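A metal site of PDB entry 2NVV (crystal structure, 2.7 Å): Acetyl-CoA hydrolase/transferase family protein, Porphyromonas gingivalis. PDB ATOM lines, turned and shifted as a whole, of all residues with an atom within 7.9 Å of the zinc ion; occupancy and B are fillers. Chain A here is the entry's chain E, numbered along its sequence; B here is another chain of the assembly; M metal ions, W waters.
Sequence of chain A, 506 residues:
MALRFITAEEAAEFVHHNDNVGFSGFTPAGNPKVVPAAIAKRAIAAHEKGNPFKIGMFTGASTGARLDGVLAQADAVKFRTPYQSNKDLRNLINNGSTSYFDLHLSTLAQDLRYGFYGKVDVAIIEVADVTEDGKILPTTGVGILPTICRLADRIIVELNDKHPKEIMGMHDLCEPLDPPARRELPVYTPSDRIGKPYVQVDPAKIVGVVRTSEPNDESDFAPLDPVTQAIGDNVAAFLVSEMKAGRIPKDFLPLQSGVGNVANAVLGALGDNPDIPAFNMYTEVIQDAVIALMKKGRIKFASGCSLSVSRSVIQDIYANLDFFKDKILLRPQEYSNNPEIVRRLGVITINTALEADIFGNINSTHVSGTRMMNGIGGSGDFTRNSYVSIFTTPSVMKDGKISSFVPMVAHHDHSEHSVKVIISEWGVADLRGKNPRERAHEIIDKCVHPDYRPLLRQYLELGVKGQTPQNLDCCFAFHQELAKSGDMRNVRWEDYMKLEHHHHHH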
ATOM      1  N   ASP A 102     -26.560 -10.312  34.492  1.00  0.00           N
ATOM      2  CA  ASP A 102     -25.858  -9.068  34.776  1.00  0.00           C
ATOM      3  C   ASP A 102     -26.267  -7.983  33.796  1.00  0.00           C
ATOM      4  O   ASP A 102     -26.377  -8.231  32.589  1.00  0.00           O
ATOM      5  CB  ASP A 102     -24.328  -9.260  34.759  1.00  0.00           C
ATOM      6  CG  ASP A 102     -23.835 -10.048  33.548  1.00  0.00           C
ATOM      7  OD1 ASP A 102     -22.674  -9.834  33.149  1.00  0.00           O
ATOM      8  OD2 ASP A 102     -24.585 -10.893  33.018  1.00  0.00           O
ATOM      9  N   ILE A 362     -13.110  -6.876  24.144  1.00  0.00           N
ATOM     10  CA  ILE A 362     -12.808  -7.216  25.527  1.00  0.00           C
ATOM     11  C   ILE A 362     -13.835  -8.125  26.209  1.00  0.00           C
ATOM     12  O   ILE A 362     -15.055  -7.988  26.035  1.00  0.00           O
ATOM     13  CB  ILE A 362     -12.626  -5.936  26.398  1.00  0.00           C
ATOM     14  CG1 ILE A 362     -11.201  -5.405  26.289  1.00  0.00           C
ATOM     15  CG2 ILE A 362     -12.899  -6.249  27.877  1.00  0.00           C
ATOM     16  CD1 ILE A 362     -10.789  -4.921  24.924  1.00  0.00           C
ATOM     17  N   ASN A 363     -13.306  -9.065  26.990  1.00  0.00           N
ATOM     18  CA  ASN A 363     -14.100 -10.002  27.765  1.00  0.00           C
ATOM     19  C   ASN A 363     -13.817  -9.622  29.206  1.00  0.00           C
ATOM     20  O   ASN A 363     -12.654  -9.610  29.635  1.00  0.00           O
ATOM     21  CB  ASN A 363     -13.631 -11.448  27.531  1.00  0.00           C
ATOM     22  CG  ASN A 363     -14.297 -12.446  28.468  1.00  0.00           C
ATOM     23  OD1 ASN A 363     -15.081 -12.076  29.364  1.00  0.00           O
ATOM     24  ND2 ASN A 363     -13.989 -13.716  28.272  1.00  0.00           N
ATOM     25  N   SER A 364     -14.854  -9.256  29.952  1.00  0.00           N
ATOM     26  CA  SER A 364     -14.643  -8.881  31.337  1.00  0.00           C
ATOM     27  C   SER A 364     -15.537  -9.666  32.292  1.00  0.00           C
ATOM     28  O   SER A 364     -15.714  -9.273  33.442  1.00  0.00           O
ATOM     29  CB  SER A 364     -14.839  -7.365  31.529  1.00  0.00           C
ATOM     30  OG  SER A 364     -15.937  -6.848  30.809  1.00  0.00           O
ATOM     31  N   THR A 365     -16.056 -10.794  31.818  1.00  0.00           N
ATOM     32  CA  THR A 365     -16.945 -11.589  32.663  1.00  0.00           C
ATOM     33  C   THR A 365     -16.843 -13.116  32.639  1.00  0.00           C
ATOM     34  O   THR A 365     -16.911 -13.743  33.689  1.00  0.00           O
ATOM     35  CB  THR A 365     -18.396 -11.223  32.371  1.00  0.00           C
ATOM     36  OG1 THR A 365     -18.621 -11.327  30.958  1.00  0.00           O
ATOM     37  CG2 THR A 365     -18.694  -9.813  32.818  1.00  0.00           C
ATOM     38  N   HIS A 366     -16.676 -13.712  31.462  1.00  0.00           N
ATOM     39  CA  HIS A 366     -16.616 -15.179  31.384  1.00  0.00           C
ATOM     40  C   HIS A 366     -15.252 -15.814  31.187  1.00  0.00           C
ATOM     41  O   HIS A 366     -14.548 -15.500  30.228  1.00  0.00           O
ATOM     42  CB  HIS A 366     -17.532 -15.672  30.262  1.00  0.00           C
ATOM     43  CG  HIS A 366     -18.985 -15.494  30.552  1.00  0.00           C
ATOM     44  ND1 HIS A 366     -19.547 -14.260  30.816  1.00  0.00           N
ATOM     45  CD2 HIS A 366     -20.001 -16.383  30.610  1.00  0.00           C
ATOM     46  CE1 HIS A 366     -20.840 -14.398  31.020  1.00  0.00           C
ATOM     47  NE2 HIS A 366     -21.146 -15.681  30.903  1.00  0.00           N
ATOM     48  N   MET A 372     -19.091 -17.672  34.644  1.00  0.00           N
ATOM     49  CA  MET A 372     -19.310 -16.302  35.073  1.00  0.00           C
ATOM     50  C   MET A 372     -18.304 -15.909  36.127  1.00  0.00           C
ATOM     51  O   MET A 372     -17.879 -16.714  36.959  1.00  0.00           O
ATOM     52  CB  MET A 372     -20.730 -16.105  35.616  1.00  0.00           C
ATOM     53  CG  MET A 372     -20.977 -14.755  36.321  1.00  0.00           C
ATOM     54  SD  MET A 372     -20.666 -13.104  35.286  1.00  0.00           S
ATOM     55  CE  MET A 372     -22.114 -13.272  33.998  1.00  0.00           C
ATOM     56  N   GLY A 375     -19.694  -9.781  36.707  1.00  0.00           N
ATOM     57  CA  GLY A 375     -20.741  -9.198  35.898  1.00  0.00           C
ATOM     58  C   GLY A 375     -20.145  -8.070  35.086  1.00  0.00           C
ATOM     59  O   GLY A 375     -19.069  -7.559  35.412  1.00  0.00           O
ATOM     60  N   ILE A 376     -20.822  -7.676  34.011  1.00  0.00           N
ATOM     61  CA  ILE A 376     -20.319  -6.612  33.162  1.00  0.00           C
ATOM     62  C   ILE A 376     -20.150  -5.325  33.980  1.00  0.00           C
ATOM     63  O   ILE A 376     -19.316  -4.481  33.652  1.00  0.00           O
ATOM     64  CB  ILE A 376     -21.250  -6.336  31.958  1.00  0.00           C
ATOM     65  CG1 ILE A 376     -20.536  -5.407  30.965  1.00  0.00           C
ATOM     66  CG2 ILE A 376     -22.584  -5.731  32.437  1.00  0.00           C
ATOM     67  CD1 ILE A 376     -21.268  -5.233  29.649  1.00  0.00           C
ATOM     68  N   HIS A 411     -15.817 -14.566  25.069  1.00  0.00           N
ATOM     69  CA  HIS A 411     -17.043 -13.879  25.491  1.00  0.00           C
ATOM     70  C   HIS A 411     -16.871 -12.394  25.237  1.00  0.00           C
ATOM     71  O   HIS A 411     -15.917 -11.785  25.731  1.00  0.00           O
ATOM     72  CB  HIS A 411     -17.323 -14.086  26.972  1.00  0.00           C
ATOM     73  CG  HIS A 411     -18.637 -13.536  27.411  1.00  0.00           C
ATOM     74  ND1 HIS A 411     -19.847 -14.119  27.077  1.00  0.00           N
ATOM     75  CD2 HIS A 411     -18.941 -12.438  28.145  1.00  0.00           C
ATOM     76  CE1 HIS A 411     -20.829 -13.402  27.582  1.00  0.00           C
ATOM     77  NE2 HIS A 411     -20.306 -12.377  28.237  1.00  0.00           N
ATOM     78  N   HIS A 412     -17.781 -11.809  24.459  1.00  0.00           N
ATOM     79  CA  HIS A 412     -17.691 -10.391  24.129  1.00  0.00           C
ATOM     80  C   HIS A 412     -18.510  -9.489  25.042  1.00  0.00           C
ATOM     81  O   HIS A 412     -19.743  -9.583  25.090  1.00  0.00           O
ATOM     82  CB  HIS A 412     -18.108 -10.141  22.671  1.00  0.00           C
ATOM     83  CG  HIS A 412     -17.194 -10.776  21.668  1.00  0.00           C
ATOM     84  ND1 HIS A 412     -16.523 -10.052  20.707  1.00  0.00           N
ATOM     85  CD2 HIS A 412     -16.865 -12.074  21.459  1.00  0.00           C
ATOM     86  CE1 HIS A 412     -15.822 -10.867  19.953  1.00  0.00           C
ATOM     87  NE2 HIS A 412     -16.002 -12.102  20.388  1.00  0.00           N
ATOM     88  N   ASP A 413     -17.818  -8.607  25.755  1.00  0.00           N
ATOM     89  CA  ASP A 413     -18.488  -7.647  26.639  1.00  0.00           C
ATOM     90  C   ASP A 413     -18.362  -6.233  26.058  1.00  0.00           C
ATOM     91  O   ASP A 413     -19.267  -5.395  26.213  1.00  0.00           O
ATOM     92  CB  ASP A 413     -17.893  -7.712  28.047  1.00  0.00           C
ATOM     93  CG  ASP A 413     -18.394  -8.896  28.835  1.00  0.00           C
ATOM     94  OD1 ASP A 413     -19.632  -9.091  28.869  1.00  0.00           O
ATOM     95  OD2 ASP A 413     -17.564  -9.635  29.421  1.00  0.00           O
ATOM     96  N   HIS A 414     -17.252  -5.959  25.400  1.00  0.00           N
ATOM     97  CA  HIS A 414     -17.024  -4.645  24.783  1.00  0.00           C
ATOM     98  C   HIS A 414     -16.480  -4.869  23.376  1.00  0.00           C
ATOM     99  O   HIS A 414     -15.589  -5.697  23.188  1.00  0.00           O
ATOM    100  CB  HIS A 414     -16.059  -3.813  25.616  1.00  0.00           C
ATOM    101  CG  HIS A 414     -16.438  -3.750  27.063  1.00  0.00           C
ATOM    102  ND1 HIS A 414     -16.028  -4.693  27.988  1.00  0.00           N
ATOM    103  CD2 HIS A 414     -17.283  -2.919  27.722  1.00  0.00           C
ATOM    104  CE1 HIS A 414     -16.600  -4.442  29.154  1.00  0.00           C
ATOM    105  NE2 HIS A 414     -17.364  -3.373  29.015  1.00  0.00           N
ATOM    106  N   ASN B 361     -26.963 -12.247  21.458  1.00  0.00           N
ATOM    107  CA  ASN B 361     -25.919 -11.418  20.882  1.00  0.00           C
ATOM    108  C   ASN B 361     -26.206 -11.233  19.405  1.00  0.00           C
ATOM    109  O   ASN B 361     -26.629 -12.182  18.734  1.00  0.00           O
ATOM    110  CB  ASN B 361     -24.561 -12.076  21.076  1.00  0.00           C
ATOM    111  CG  ASN B 361     -24.227 -12.302  22.533  1.00  0.00           C
ATOM    112  OD1 ASN B 361     -23.828 -11.377  23.237  1.00  0.00           O
ATOM    113  ND2 ASN B 361     -24.409 -13.532  22.997  1.00  0.00           N
ATOM    114  N   SER B 415     -24.289  -6.844  22.481  1.00  0.00           N
ATOM    115  CA  SER B 415     -24.231  -7.902  23.482  1.00  0.00           C
ATOM    116  C   SER B 415     -25.539  -8.219  24.224  1.00  0.00           C
ATOM    117  O   SER B 415     -26.491  -7.453  24.215  1.00  0.00           O
ATOM    118  CB  SER B 415     -23.159  -7.574  24.522  1.00  0.00           C
ATOM    119  OG  SER B 415     -23.672  -6.697  25.513  1.00  0.00           O
ATOM    120  N   GLU B 416     -25.528  -9.371  24.892  1.00  0.00           N
ATOM    121  CA  GLU B 416     -26.649  -9.851  25.676  1.00  0.00           C
ATOM    122  C   GLU B 416     -27.179  -8.811  26.648  1.00  0.00           C
ATOM    123  O   GLU B 416     -28.332  -8.874  27.082  1.00  0.00           O
ATOM    124  CB  GLU B 416     -26.212 -11.094  26.462  1.00  0.00           C
ATOM    125  CG  GLU B 416     -24.963 -10.866  27.329  1.00  0.00           C
ATOM    126  CD  GLU B 416     -24.684 -12.029  28.262  1.00  0.00           C
ATOM    127  OE1 GLU B 416     -23.614 -12.059  28.875  1.00  0.00           O
ATOM    128  OE2 GLU B 416     -25.546 -12.907  28.371  1.00  0.00           O
ATOM    129  N   HIS B 417     -26.317  -7.860  27.015  1.00  0.00           N
ATOM    130  CA  HIS B 417     -26.669  -6.812  27.968  1.00  0.00           C
ATOM    131  C   HIS B 417     -27.394  -5.658  27.318  1.00  0.00           C
ATOM    132  O   HIS B 417     -27.930  -4.798  27.995  1.00  0.00           O
ATOM    133  CB  HIS B 417     -25.394  -6.270  28.629  1.00  0.00           C
ATOM    134  CG  HIS B 417     -24.522  -7.328  29.222  1.00  0.00           C
ATOM    135  ND1 HIS B 417     -24.886  -8.052  30.328  1.00  0.00           N
ATOM    136  CD2 HIS B 417     -23.336  -7.819  28.825  1.00  0.00           C
ATOM    137  CE1 HIS B 417     -23.953  -8.948  30.592  1.00  0.00           C
ATOM    138  NE2 HIS B 417     -22.998  -8.824  29.685  1.00  0.00           N
ATOM    139  N   ARG B 439     -33.012 -17.456  27.956  1.00  0.00           N
ATOM    140  CA  ARG B 439     -33.247 -16.666  26.754  1.00  0.00           C
ATOM    141  C   ARG B 439     -32.934 -17.485  25.494  1.00  0.00           C
ATOM    142  O   ARG B 439     -33.440 -17.206  24.401  1.00  0.00           O
ATOM    143  CB  ARG B 439     -32.466 -15.342  26.807  1.00  0.00           C
ATOM    144  CG  ARG B 439     -31.003 -15.401  26.497  1.00  0.00           C
ATOM    145  CD  ARG B 439     -30.418 -13.974  26.497  1.00  0.00           C
ATOM    146  NE  ARG B 439     -30.161 -13.463  27.832  1.00  0.00           N
ATOM    147  CZ  ARG B 439     -28.990 -13.595  28.450  1.00  0.00           C
ATOM    148  NH1 ARG B 439     -28.830 -13.107  29.680  1.00  0.00           N
ATOM    149  NH2 ARG B 439     -27.987 -14.194  27.844  1.00  0.00           N
ATOM    150  N   THR B 468     -22.828 -19.460  30.944  1.00  0.00           N
ATOM    151  CA  THR B 468     -23.095 -19.506  29.518  1.00  0.00           C
ATOM    152  C   THR B 468     -22.586 -20.817  28.907  1.00  0.00           C
ATOM    153  O   THR B 468     -21.380 -21.087  28.879  1.00  0.00           O
ATOM    154  CB  THR B 468     -22.424 -18.296  28.819  1.00  0.00           C
ATOM    155  OG1 THR B 468     -22.892 -17.095  29.452  1.00  0.00           O
ATOM    156  CG2 THR B 468     -22.770 -18.268  27.313  1.00  0.00           C
HETATM  157 ZN    ZN M   1     -21.354 -10.411  28.930  1.00  0.00          ZN
HETATM  158  O   HOH W   1     -21.162 -10.743  31.474  1.00  0.00           O
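OD2 of Asp 413 sits at hydrogen-bond distance from OG1 of Thr 365, 2.5 Å away. N of Ser 364 is in hydrogen-bond range of OD2 of Asp 413 (2.8 Å). N of Asp 413 lies within hydrogen-bond range of O of Ile 362. A ring nitrogen (NE2) of His 417 of chain B lies close to the side-chain carboxylate of Glu 416 of chain B, at 3.4 Å. ND1 of His 417 of chain B is in hydrogen-bond range of O of Asp 102 (2.7 Å). N of Glu 416 of chain B lies within hydrogen-bond range of OD1 of Asn 361 of chain B (3.1 Å). NH2 of Arg 439 of chain B is in salt-bridge range of OE2 of Glu 416 of chain B, 2.8 Å away. OG1 of Thr 365 is in hydrogen-bond range of ND1 of His 366.
Thr 365 touches the zinc ion. Five residues have an atom within 4 Å of the zinc ion: Thr 365, His 411, Asp 413, Glu 416 of chain B and His 417 of chain B. Along chain A the residues within 4 Å of the zinc ion span positions 365 to 413.
Water W1 lies within hydrogen-bond range of OD1 of Asp 102 (2.4 Å) and OG1 of Thr 365 (2.7 Å).
The zinc ion is bound by the side-chain carboxylate (OD1) of Asp 413 (2.2 Å), a ring nitrogen (NE2) of His 411 (2.3 Å), a ring nitrogen (NE2) of His 417 of chain B (2.4 Å) and water W1 (2.6 Å). The zinc ion has four donor atoms within binding distance. Slightly farther from the zinc ion lies OE1 of Glu 416 of chain B (2.8 Å).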
